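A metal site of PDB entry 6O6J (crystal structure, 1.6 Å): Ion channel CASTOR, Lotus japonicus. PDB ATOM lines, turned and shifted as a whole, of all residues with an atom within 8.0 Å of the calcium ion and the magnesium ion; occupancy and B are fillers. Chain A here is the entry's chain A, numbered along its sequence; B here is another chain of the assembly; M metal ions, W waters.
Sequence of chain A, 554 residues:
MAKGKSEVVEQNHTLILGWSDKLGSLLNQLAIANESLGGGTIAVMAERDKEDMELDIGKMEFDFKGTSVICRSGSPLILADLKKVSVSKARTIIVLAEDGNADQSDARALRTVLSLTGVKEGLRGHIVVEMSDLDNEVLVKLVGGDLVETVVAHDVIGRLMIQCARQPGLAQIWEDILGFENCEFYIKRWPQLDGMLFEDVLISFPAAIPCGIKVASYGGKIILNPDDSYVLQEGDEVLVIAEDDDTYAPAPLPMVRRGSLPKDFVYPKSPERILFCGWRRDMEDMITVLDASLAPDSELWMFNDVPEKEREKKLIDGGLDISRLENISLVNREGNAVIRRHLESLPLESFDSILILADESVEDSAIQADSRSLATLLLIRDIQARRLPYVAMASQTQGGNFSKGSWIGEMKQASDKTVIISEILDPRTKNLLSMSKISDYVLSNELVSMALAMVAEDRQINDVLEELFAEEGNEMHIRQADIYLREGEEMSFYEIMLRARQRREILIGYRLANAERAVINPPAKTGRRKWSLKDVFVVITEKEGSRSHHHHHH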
ATOM      1  N   ALA A 102      21.618 -22.294 -14.496  1.00  0.00           N
ATOM      2  CA  ALA A 102      20.179 -22.062 -14.671  1.00  0.00           C
ATOM      3  C   ALA A 102      19.888 -21.045 -15.765  1.00  0.00           C
ATOM      4  O   ALA A 102      18.925 -21.195 -16.525  1.00  0.00           O
ATOM      5  CB  ALA A 102      19.565 -21.592 -13.348  1.00  0.00           C
ATOM      6  N   ASP A 103      20.644 -19.945 -15.831  1.00  0.00           N
ATOM      7  CA  ASP A 103      20.348 -18.952 -16.866  1.00  0.00           C
ATOM      8  C   ASP A 103      20.559 -19.510 -18.271  1.00  0.00           C
ATOM      9  O   ASP A 103      19.796 -19.209 -19.191  1.00  0.00           O
ATOM     10  CB  ASP A 103      21.191 -17.694 -16.657  1.00  0.00           C
ATOM     11  CG  ASP A 103      20.612 -16.734 -15.609  1.00  0.00           C
ATOM     12  OD1 ASP A 103      19.392 -16.811 -15.292  1.00  0.00           O
ATOM     13  OD2 ASP A 103      21.391 -15.901 -15.100  1.00  0.00           O
ATOM     14  N   ASP A 106      17.660 -21.748 -19.092  1.00  0.00           N
ATOM     15  CA  ASP A 106      16.452 -20.998 -19.402  1.00  0.00           C
ATOM     16  C   ASP A 106      16.539 -20.260 -20.740  1.00  0.00           C
ATOM     17  O   ASP A 106      15.522 -20.042 -21.416  1.00  0.00           O
ATOM     18  CB  ASP A 106      16.169 -20.023 -18.262  1.00  0.00           C
ATOM     19  CG  ASP A 106      15.543 -20.717 -17.050  1.00  0.00           C
ATOM     20  OD1 ASP A 106      15.186 -21.922 -17.125  1.00  0.00           O
ATOM     21  OD2 ASP A 106      15.448 -20.050 -16.012  1.00  0.00           O
ATOM     22  N   SER A 132      14.323 -23.082 -14.860  1.00  0.00           N
ATOM     23  CA  SER A 132      15.265 -23.234 -13.764  1.00  0.00           C
ATOM     24  C   SER A 132      15.313 -22.031 -12.833  1.00  0.00           C
ATOM     25  O   SER A 132      15.840 -22.169 -11.718  1.00  0.00           O
ATOM     26  CB  SER A 132      16.670 -23.493 -14.316  1.00  0.00           C
ATOM     27  OG  SER A 132      16.671 -24.690 -15.098  1.00  0.00           O
ATOM     28  N   ASP A 133      14.793 -20.875 -13.241  1.00  0.00           N
ATOM     29  CA  ASP A 133      14.878 -19.651 -12.460  1.00  0.00           C
ATOM     30  C   ASP A 133      13.583 -18.869 -12.638  1.00  0.00           C
ATOM     31  O   ASP A 133      13.162 -18.600 -13.753  1.00  0.00           O
ATOM     32  CB  ASP A 133      16.126 -18.835 -12.876  1.00  0.00           C
ATOM     33  CG  ASP A 133      16.443 -17.667 -11.928  1.00  0.00           C
ATOM     34  OD1 ASP A 133      15.611 -16.774 -11.777  1.00  0.00           O
ATOM     35  OD2 ASP A 133      17.535 -17.652 -11.329  1.00  0.00           O
ATOM     36  N   LEU A 134      12.960 -18.516 -11.514  1.00  0.00           N
ATOM     37  CA  LEU A 134      11.686 -17.824 -11.538  1.00  0.00           C
ATOM     38  C   LEU A 134      11.773 -16.500 -12.320  1.00  0.00           C
ATOM     39  O   LEU A 134      10.790 -16.099 -12.964  1.00  0.00           O
ATOM     40  CB  LEU A 134      11.247 -17.554 -10.117  1.00  0.00           C
ATOM     41  CG  LEU A 134       9.891 -16.898  -9.920  1.00  0.00           C
ATOM     42  CD1 LEU A 134       8.798 -17.781 -10.448  1.00  0.00           C
ATOM     43  CD2 LEU A 134       9.706 -16.679  -8.417  1.00  0.00           C
ATOM     44  N   ASP A 135      12.914 -15.841 -12.275  1.00  0.00           N
ATOM     45  CA  ASP A 135      13.035 -14.538 -12.936  1.00  0.00           C
ATOM     46  C   ASP A 135      12.950 -14.629 -14.454  1.00  0.00           C
ATOM     47  O   ASP A 135      12.818 -13.597 -15.129  1.00  0.00           O
ATOM     48  CB  ASP A 135      14.342 -13.881 -12.500  1.00  0.00           C
ATOM     49  CG  ASP A 135      14.367 -13.571 -11.001  1.00  0.00           C
ATOM     50  OD1 ASP A 135      13.477 -12.803 -10.567  1.00  0.00           O
ATOM     51  OD2 ASP A 135      15.278 -14.085 -10.295  1.00  0.00           O
ATOM     52  N   ASN A 136      13.008 -15.831 -15.016  1.00  0.00           N
ATOM     53  CA  ASN A 136      12.943 -16.022 -16.457  1.00  0.00           C
ATOM     54  C   ASN A 136      11.570 -16.545 -16.894  1.00  0.00           C
ATOM     55  O   ASN A 136      11.312 -16.665 -18.107  1.00  0.00           O
ATOM     56  CB  ASN A 136      14.051 -16.990 -16.893  1.00  0.00           C
ATOM     57  CG  ASN A 136      15.444 -16.431 -16.635  1.00  0.00           C
ATOM     58  OD1 ASN A 136      15.671 -15.240 -16.878  1.00  0.00           O
ATOM     59  ND2 ASN A 136      16.351 -17.251 -16.131  1.00  0.00           N
ATOM     60  N   HIS A 154      13.200 -25.064  -9.618  1.00  0.00           N
ATOM     61  CA  HIS A 154      13.886 -24.565  -8.439  1.00  0.00           C
ATOM     62  C   HIS A 154      12.904 -24.019  -7.398  1.00  0.00           C
ATOM     63  O   HIS A 154      13.058 -24.240  -6.181  1.00  0.00           O
ATOM     64  CB  HIS A 154      14.842 -23.468  -8.929  1.00  0.00           C
ATOM     65  CG  HIS A 154      15.778 -22.953  -7.906  1.00  0.00           C
ATOM     66  ND1 HIS A 154      16.754 -23.724  -7.334  1.00  0.00           N
ATOM     67  CD2 HIS A 154      15.911 -21.709  -7.381  1.00  0.00           C
ATOM     68  CE1 HIS A 154      17.449 -22.986  -6.480  1.00  0.00           C
ATOM     69  NE2 HIS A 154      16.956 -21.762  -6.488  1.00  0.00           N
ATOM     70  N   ASP A 155      11.885 -23.306  -7.869  1.00  0.00           N
ATOM     71  CA  ASP A 155      10.930 -22.680  -6.981  1.00  0.00           C
ATOM     72  C   ASP A 155      10.005 -23.710  -6.346  1.00  0.00           C
ATOM     73  O   ASP A 155       9.717 -23.631  -5.133  1.00  0.00           O
ATOM     74  CB  ASP A 155      10.119 -21.643  -7.787  1.00  0.00           C
ATOM     75  CG  ASP A 155       9.232 -20.771  -6.913  1.00  0.00           C
ATOM     76  OD1 ASP A 155       9.739 -19.754  -6.345  1.00  0.00           O
ATOM     77  OD2 ASP A 155       8.040 -21.096  -6.808  1.00  0.00           O
ATOM     78  N   ARG A 281      20.273 -20.079  -4.521  1.00  0.00           N
ATOM     79  CA  ARG A 281      19.916 -19.080  -5.521  1.00  0.00           C
ATOM     80  C   ARG A 281      18.468 -18.645  -5.319  1.00  0.00           C
ATOM     81  O   ARG A 281      17.596 -19.474  -5.035  1.00  0.00           O
ATOM     82  CB  ARG A 281      20.106 -19.649  -6.940  1.00  0.00           C
ATOM     83  CG  ARG A 281      19.631 -18.692  -8.038  1.00  0.00           C
ATOM     84  CD  ARG A 281      20.088 -19.187  -9.438  1.00  0.00           C
ATOM     85  NE  ARG A 281      19.911 -20.632  -9.584  1.00  0.00           N
ATOM     86  CZ  ARG A 281      18.774 -21.196  -9.961  1.00  0.00           C
ATOM     87  NH1 ARG A 281      17.718 -20.444 -10.256  1.00  0.00           N
ATOM     88  NH2 ARG A 281      18.680 -22.516 -10.049  1.00  0.00           N
ATOM     89  N   ASP A 282      18.238 -17.330  -5.387  1.00  0.00           N
ATOM     90  CA  ASP A 282      16.911 -16.738  -5.186  1.00  0.00           C
ATOM     91  C   ASP A 282      16.305 -17.088  -3.817  1.00  0.00           C
ATOM     92  O   ASP A 282      15.090 -17.213  -3.702  1.00  0.00           O
ATOM     93  CB  ASP A 282      15.953 -17.161  -6.321  1.00  0.00           C
ATOM     94  CG  ASP A 282      16.335 -16.538  -7.679  1.00  0.00           C
ATOM     95  OD1 ASP A 282      17.214 -15.654  -7.725  1.00  0.00           O
ATOM     96  OD2 ASP A 282      15.810 -16.980  -8.712  1.00  0.00           O
ATOM     97  N   MET A 283      17.141 -17.216  -2.786  1.00  0.00           N
ATOM     98  CA  MET A 283      16.642 -17.595  -1.449  1.00  0.00           C
ATOM     99  C   MET A 283      15.583 -16.631  -0.914  1.00  0.00           C
ATOM    100  O   MET A 283      14.783 -17.031  -0.066  1.00  0.00           O
ATOM    101  CB  MET A 283      17.789 -17.691  -0.454  1.00  0.00           C
ATOM    102  CG  MET A 283      17.395 -18.497   0.808  1.00  0.00           C
ATOM    103  SD  MET A 283      18.820 -19.129   1.665  1.00  0.00           S
ATOM    104  CE  MET A 283      19.600 -17.589   2.176  1.00  0.00           C
ATOM    105  N   GLU A 284      15.583 -15.367  -1.375  1.00  0.00           N
ATOM    106  CA  GLU A 284      14.542 -14.427  -0.952  1.00  0.00           C
ATOM    107  C   GLU A 284      13.133 -14.963  -1.232  1.00  0.00           C
ATOM    108  O   GLU A 284      12.184 -14.650  -0.511  1.00  0.00           O
ATOM    109  CB  GLU A 284      14.737 -13.061  -1.637  1.00  0.00           C
ATOM    110  CG  GLU A 284      14.638 -13.119  -3.157  1.00  0.00           C
ATOM    111  CD  GLU A 284      15.956 -13.473  -3.875  1.00  0.00           C
ATOM    112  OE1 GLU A 284      16.938 -13.880  -3.209  1.00  0.00           O
ATOM    113  OE2 GLU A 284      16.013 -13.322  -5.115  1.00  0.00           O
ATOM    114  N   ASP A 285      12.989 -15.765  -2.285  1.00  0.00           N
ATOM    115  CA  ASP A 285      11.677 -16.329  -2.599  1.00  0.00           C
ATOM    116  C   ASP A 285      11.223 -17.307  -1.512  1.00  0.00           C
ATOM    117  O   ASP A 285      10.046 -17.308  -1.121  1.00  0.00           O
ATOM    118  CB  ASP A 285      11.721 -17.019  -3.976  1.00  0.00           C
ATOM    119  CG  ASP A 285      12.037 -16.026  -5.129  1.00  0.00           C
ATOM    120  OD1 ASP A 285      11.773 -14.814  -4.958  1.00  0.00           O
ATOM    121  OD2 ASP A 285      12.533 -16.453  -6.193  1.00  0.00           O
ATOM    122  N   ASP A 317      17.821  -6.755  -3.617  1.00  0.00           N
ATOM    123  CA  ASP A 317      17.903  -6.873  -5.076  1.00  0.00           C
ATOM    124  C   ASP A 317      16.992  -7.977  -5.591  1.00  0.00           C
ATOM    125  O   ASP A 317      16.515  -7.900  -6.724  1.00  0.00           O
ATOM    126  CB  ASP A 317      19.356  -7.133  -5.486  1.00  0.00           C
ATOM    127  CG  ASP A 317      20.203  -5.870  -5.433  1.00  0.00           C
ATOM    128  OD1 ASP A 317      19.665  -4.798  -5.072  1.00  0.00           O
ATOM    129  OD2 ASP A 317      21.411  -5.963  -5.727  1.00  0.00           O
ATOM    130  N   GLY A 318      16.737  -9.000  -4.776  1.00  0.00           N
ATOM    131  CA  GLY A 318      15.769 -10.013  -5.141  1.00  0.00           C
ATOM    132  C   GLY A 318      14.332  -9.674  -4.820  1.00  0.00           C
ATOM    133  O   GLY A 318      13.451 -10.533  -4.967  1.00  0.00           O
ATOM    134  N   GLY A 319      14.046  -8.450  -4.374  1.00  0.00           N
ATOM    135  CA  GLY A 319      12.679  -8.016  -4.185  1.00  0.00           C
ATOM    136  C   GLY A 319      12.141  -8.110  -2.780  1.00  0.00           C
ATOM    137  O   GLY A 319      10.965  -7.797  -2.555  1.00  0.00           O
ATOM    138  N   LEU A 320      12.958  -8.505  -1.812  1.00  0.00           N
ATOM    139  CA  LEU A 320      12.480  -8.721  -0.449  1.00  0.00           C
ATOM    140  C   LEU A 320      12.844  -7.524   0.413  1.00  0.00           C
ATOM    141  O   LEU A 320      14.021  -7.149   0.510  1.00  0.00           O
ATOM    142  CB  LEU A 320      13.097  -9.993   0.143  1.00  0.00           C
ATOM    143  CG  LEU A 320      12.741 -10.255   1.608  1.00  0.00           C
ATOM    144  CD1 LEU A 320      11.255 -10.404   1.801  1.00  0.00           C
ATOM    145  CD2 LEU A 320      13.458 -11.493   2.114  1.00  0.00           C
ATOM    146  N   GLU A 360      24.219 -21.617  -3.927  1.00  0.00           N
ATOM    147  CA  GLU A 360      24.336 -21.052  -5.276  1.00  0.00           C
ATOM    148  C   GLU A 360      25.767 -21.112  -5.797  1.00  0.00           C
ATOM    149  O   GLU A 360      25.970 -21.104  -7.029  1.00  0.00           O
ATOM    150  CB  GLU A 360      23.833 -19.611  -5.310  1.00  0.00           C
ATOM    151  CG  GLU A 360      24.655 -18.633  -4.505  1.00  0.00           C
ATOM    152  CD  GLU A 360      24.133 -17.195  -4.652  1.00  0.00           C
ATOM    153  OE1 GLU A 360      23.155 -16.989  -5.412  1.00  0.00           O
ATOM    154  OE2 GLU A 360      24.710 -16.289  -4.021  1.00  0.00           O
ATOM    155  N   VAL B 338      19.844  -6.403 -15.150  1.00  0.00           N
ATOM    156  CA  VAL B 338      18.772  -7.391 -15.043  1.00  0.00           C
ATOM    157  C   VAL B 338      18.139  -7.397 -13.657  1.00  0.00           C
ATOM    158  O   VAL B 338      17.353  -8.312 -13.340  1.00  0.00           O
ATOM    159  CB  VAL B 338      19.237  -8.799 -15.456  1.00  0.00           C
ATOM    160  CG1 VAL B 338      19.836  -8.760 -16.872  1.00  0.00           C
ATOM    161  CG2 VAL B 338      20.221  -9.381 -14.420  1.00  0.00           C
ATOM    162  N   ILE B 339      18.399  -6.377 -12.835  1.00  0.00           N
ATOM    163  CA  ILE B 339      17.855  -6.293 -11.490  1.00  0.00           C
ATOM    164  C   ILE B 339      16.787  -5.206 -11.507  1.00  0.00           C
ATOM    165  O   ILE B 339      17.094  -4.020 -11.686  1.00  0.00           O
ATOM    166  CB  ILE B 339      18.934  -5.991 -10.454  1.00  0.00           C
ATOM    167  CG1 ILE B 339      20.001  -7.085 -10.444  1.00  0.00           C
ATOM    168  CG2 ILE B 339      18.279  -5.791  -9.080  1.00  0.00           C
ATOM    169  CD1 ILE B 339      19.464  -8.461 -10.177  1.00  0.00           C
ATOM    170  N   ARG B 340      15.533  -5.635 -11.290  1.00  0.00           N
ATOM    171  CA  ARG B 340      14.406  -4.705 -11.334  1.00  0.00           C
ATOM    172  C   ARG B 340      14.628  -3.501 -10.438  1.00  0.00           C
ATOM    173  O   ARG B 340      14.411  -2.359 -10.858  1.00  0.00           O
ATOM    174  CB  ARG B 340      13.114  -5.435 -10.959  1.00  0.00           C
ATOM    175  CG  ARG B 340      11.892  -4.512 -10.932  1.00  0.00           C
ATOM    176  CD  ARG B 340      10.659  -5.236 -10.379  1.00  0.00           C
ATOM    177  NE  ARG B 340      10.263  -6.336 -11.268  1.00  0.00           N
ATOM    178  CZ  ARG B 340       9.407  -6.209 -12.278  1.00  0.00           C
ATOM    179  NH1 ARG B 340       8.816  -5.037 -12.510  1.00  0.00           N
ATOM    180  NH2 ARG B 340       9.100  -7.260 -13.041  1.00  0.00           N
HETATM  181 CA    CA M   1      17.084 -15.516 -10.206  1.00  0.00          CA
HETATM  182 MG    MG M   2      13.152 -12.833  -8.329  1.00  0.00          MG
HETATM  183  O   HOH W   1      15.342 -12.682  -7.924  1.00  0.00           O
HETATM  184  O   HOH W   2      13.330 -10.964  -8.321  1.00  0.00           O
HETATM  185  O   HOH W   3      11.123 -12.893  -8.760  1.00  0.00           O
HETATM  186  O   HOH W   4      13.151 -14.891  -8.149  1.00  0.00           O
HETATM  187  O   HOH W   5      17.790 -14.635 -12.313  1.00  0.00           O
HETATM  188  O   HOH W   6      19.596 -15.873  -9.812  1.00  0.00           O
HETATM  189  O   HOH W   7      17.807 -13.286  -9.514  1.00  0.00           O
HETATM  190  O   HOH W   8      12.668 -12.919  -6.343  1.00  0.00           O
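The side-chain carboxylate (OD2) of Asp 133 lies close to the guanidinium group (NH1) of Arg 281. The backbone NH of Asp 133 lies within hydrogen-bond range of the side-chain carboxylate of Asp 106 (3.0 Å).
Within 4 Å of the magnesium ion: Asp 135.
The calcium ion is bound by the side-chain carboxylate (OD2) of Asp 135 (2.3 Å), water W5 (2.4 Å), water W7 (2.4 Å), the side-chain carboxylate (OD2) of Asp 282 (2.4 Å), the side-chain carboxylate (OD2) of Asp 133 (2.5 Å), the side-chain carboxylate (OD1) of Asp 282 (2.5 Å), the side-chain carboxylate (OD1) of Asp 133 (2.5 Å) and water W6 (2.6 Å).
The magnesium ion is bound by water W2, water W8, water W4, water W3, water W1 and OD1 of Asp 135.
Water W8 lies within hydrogen-bond range of OD1 of Asp 285 and O of Gly 318.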
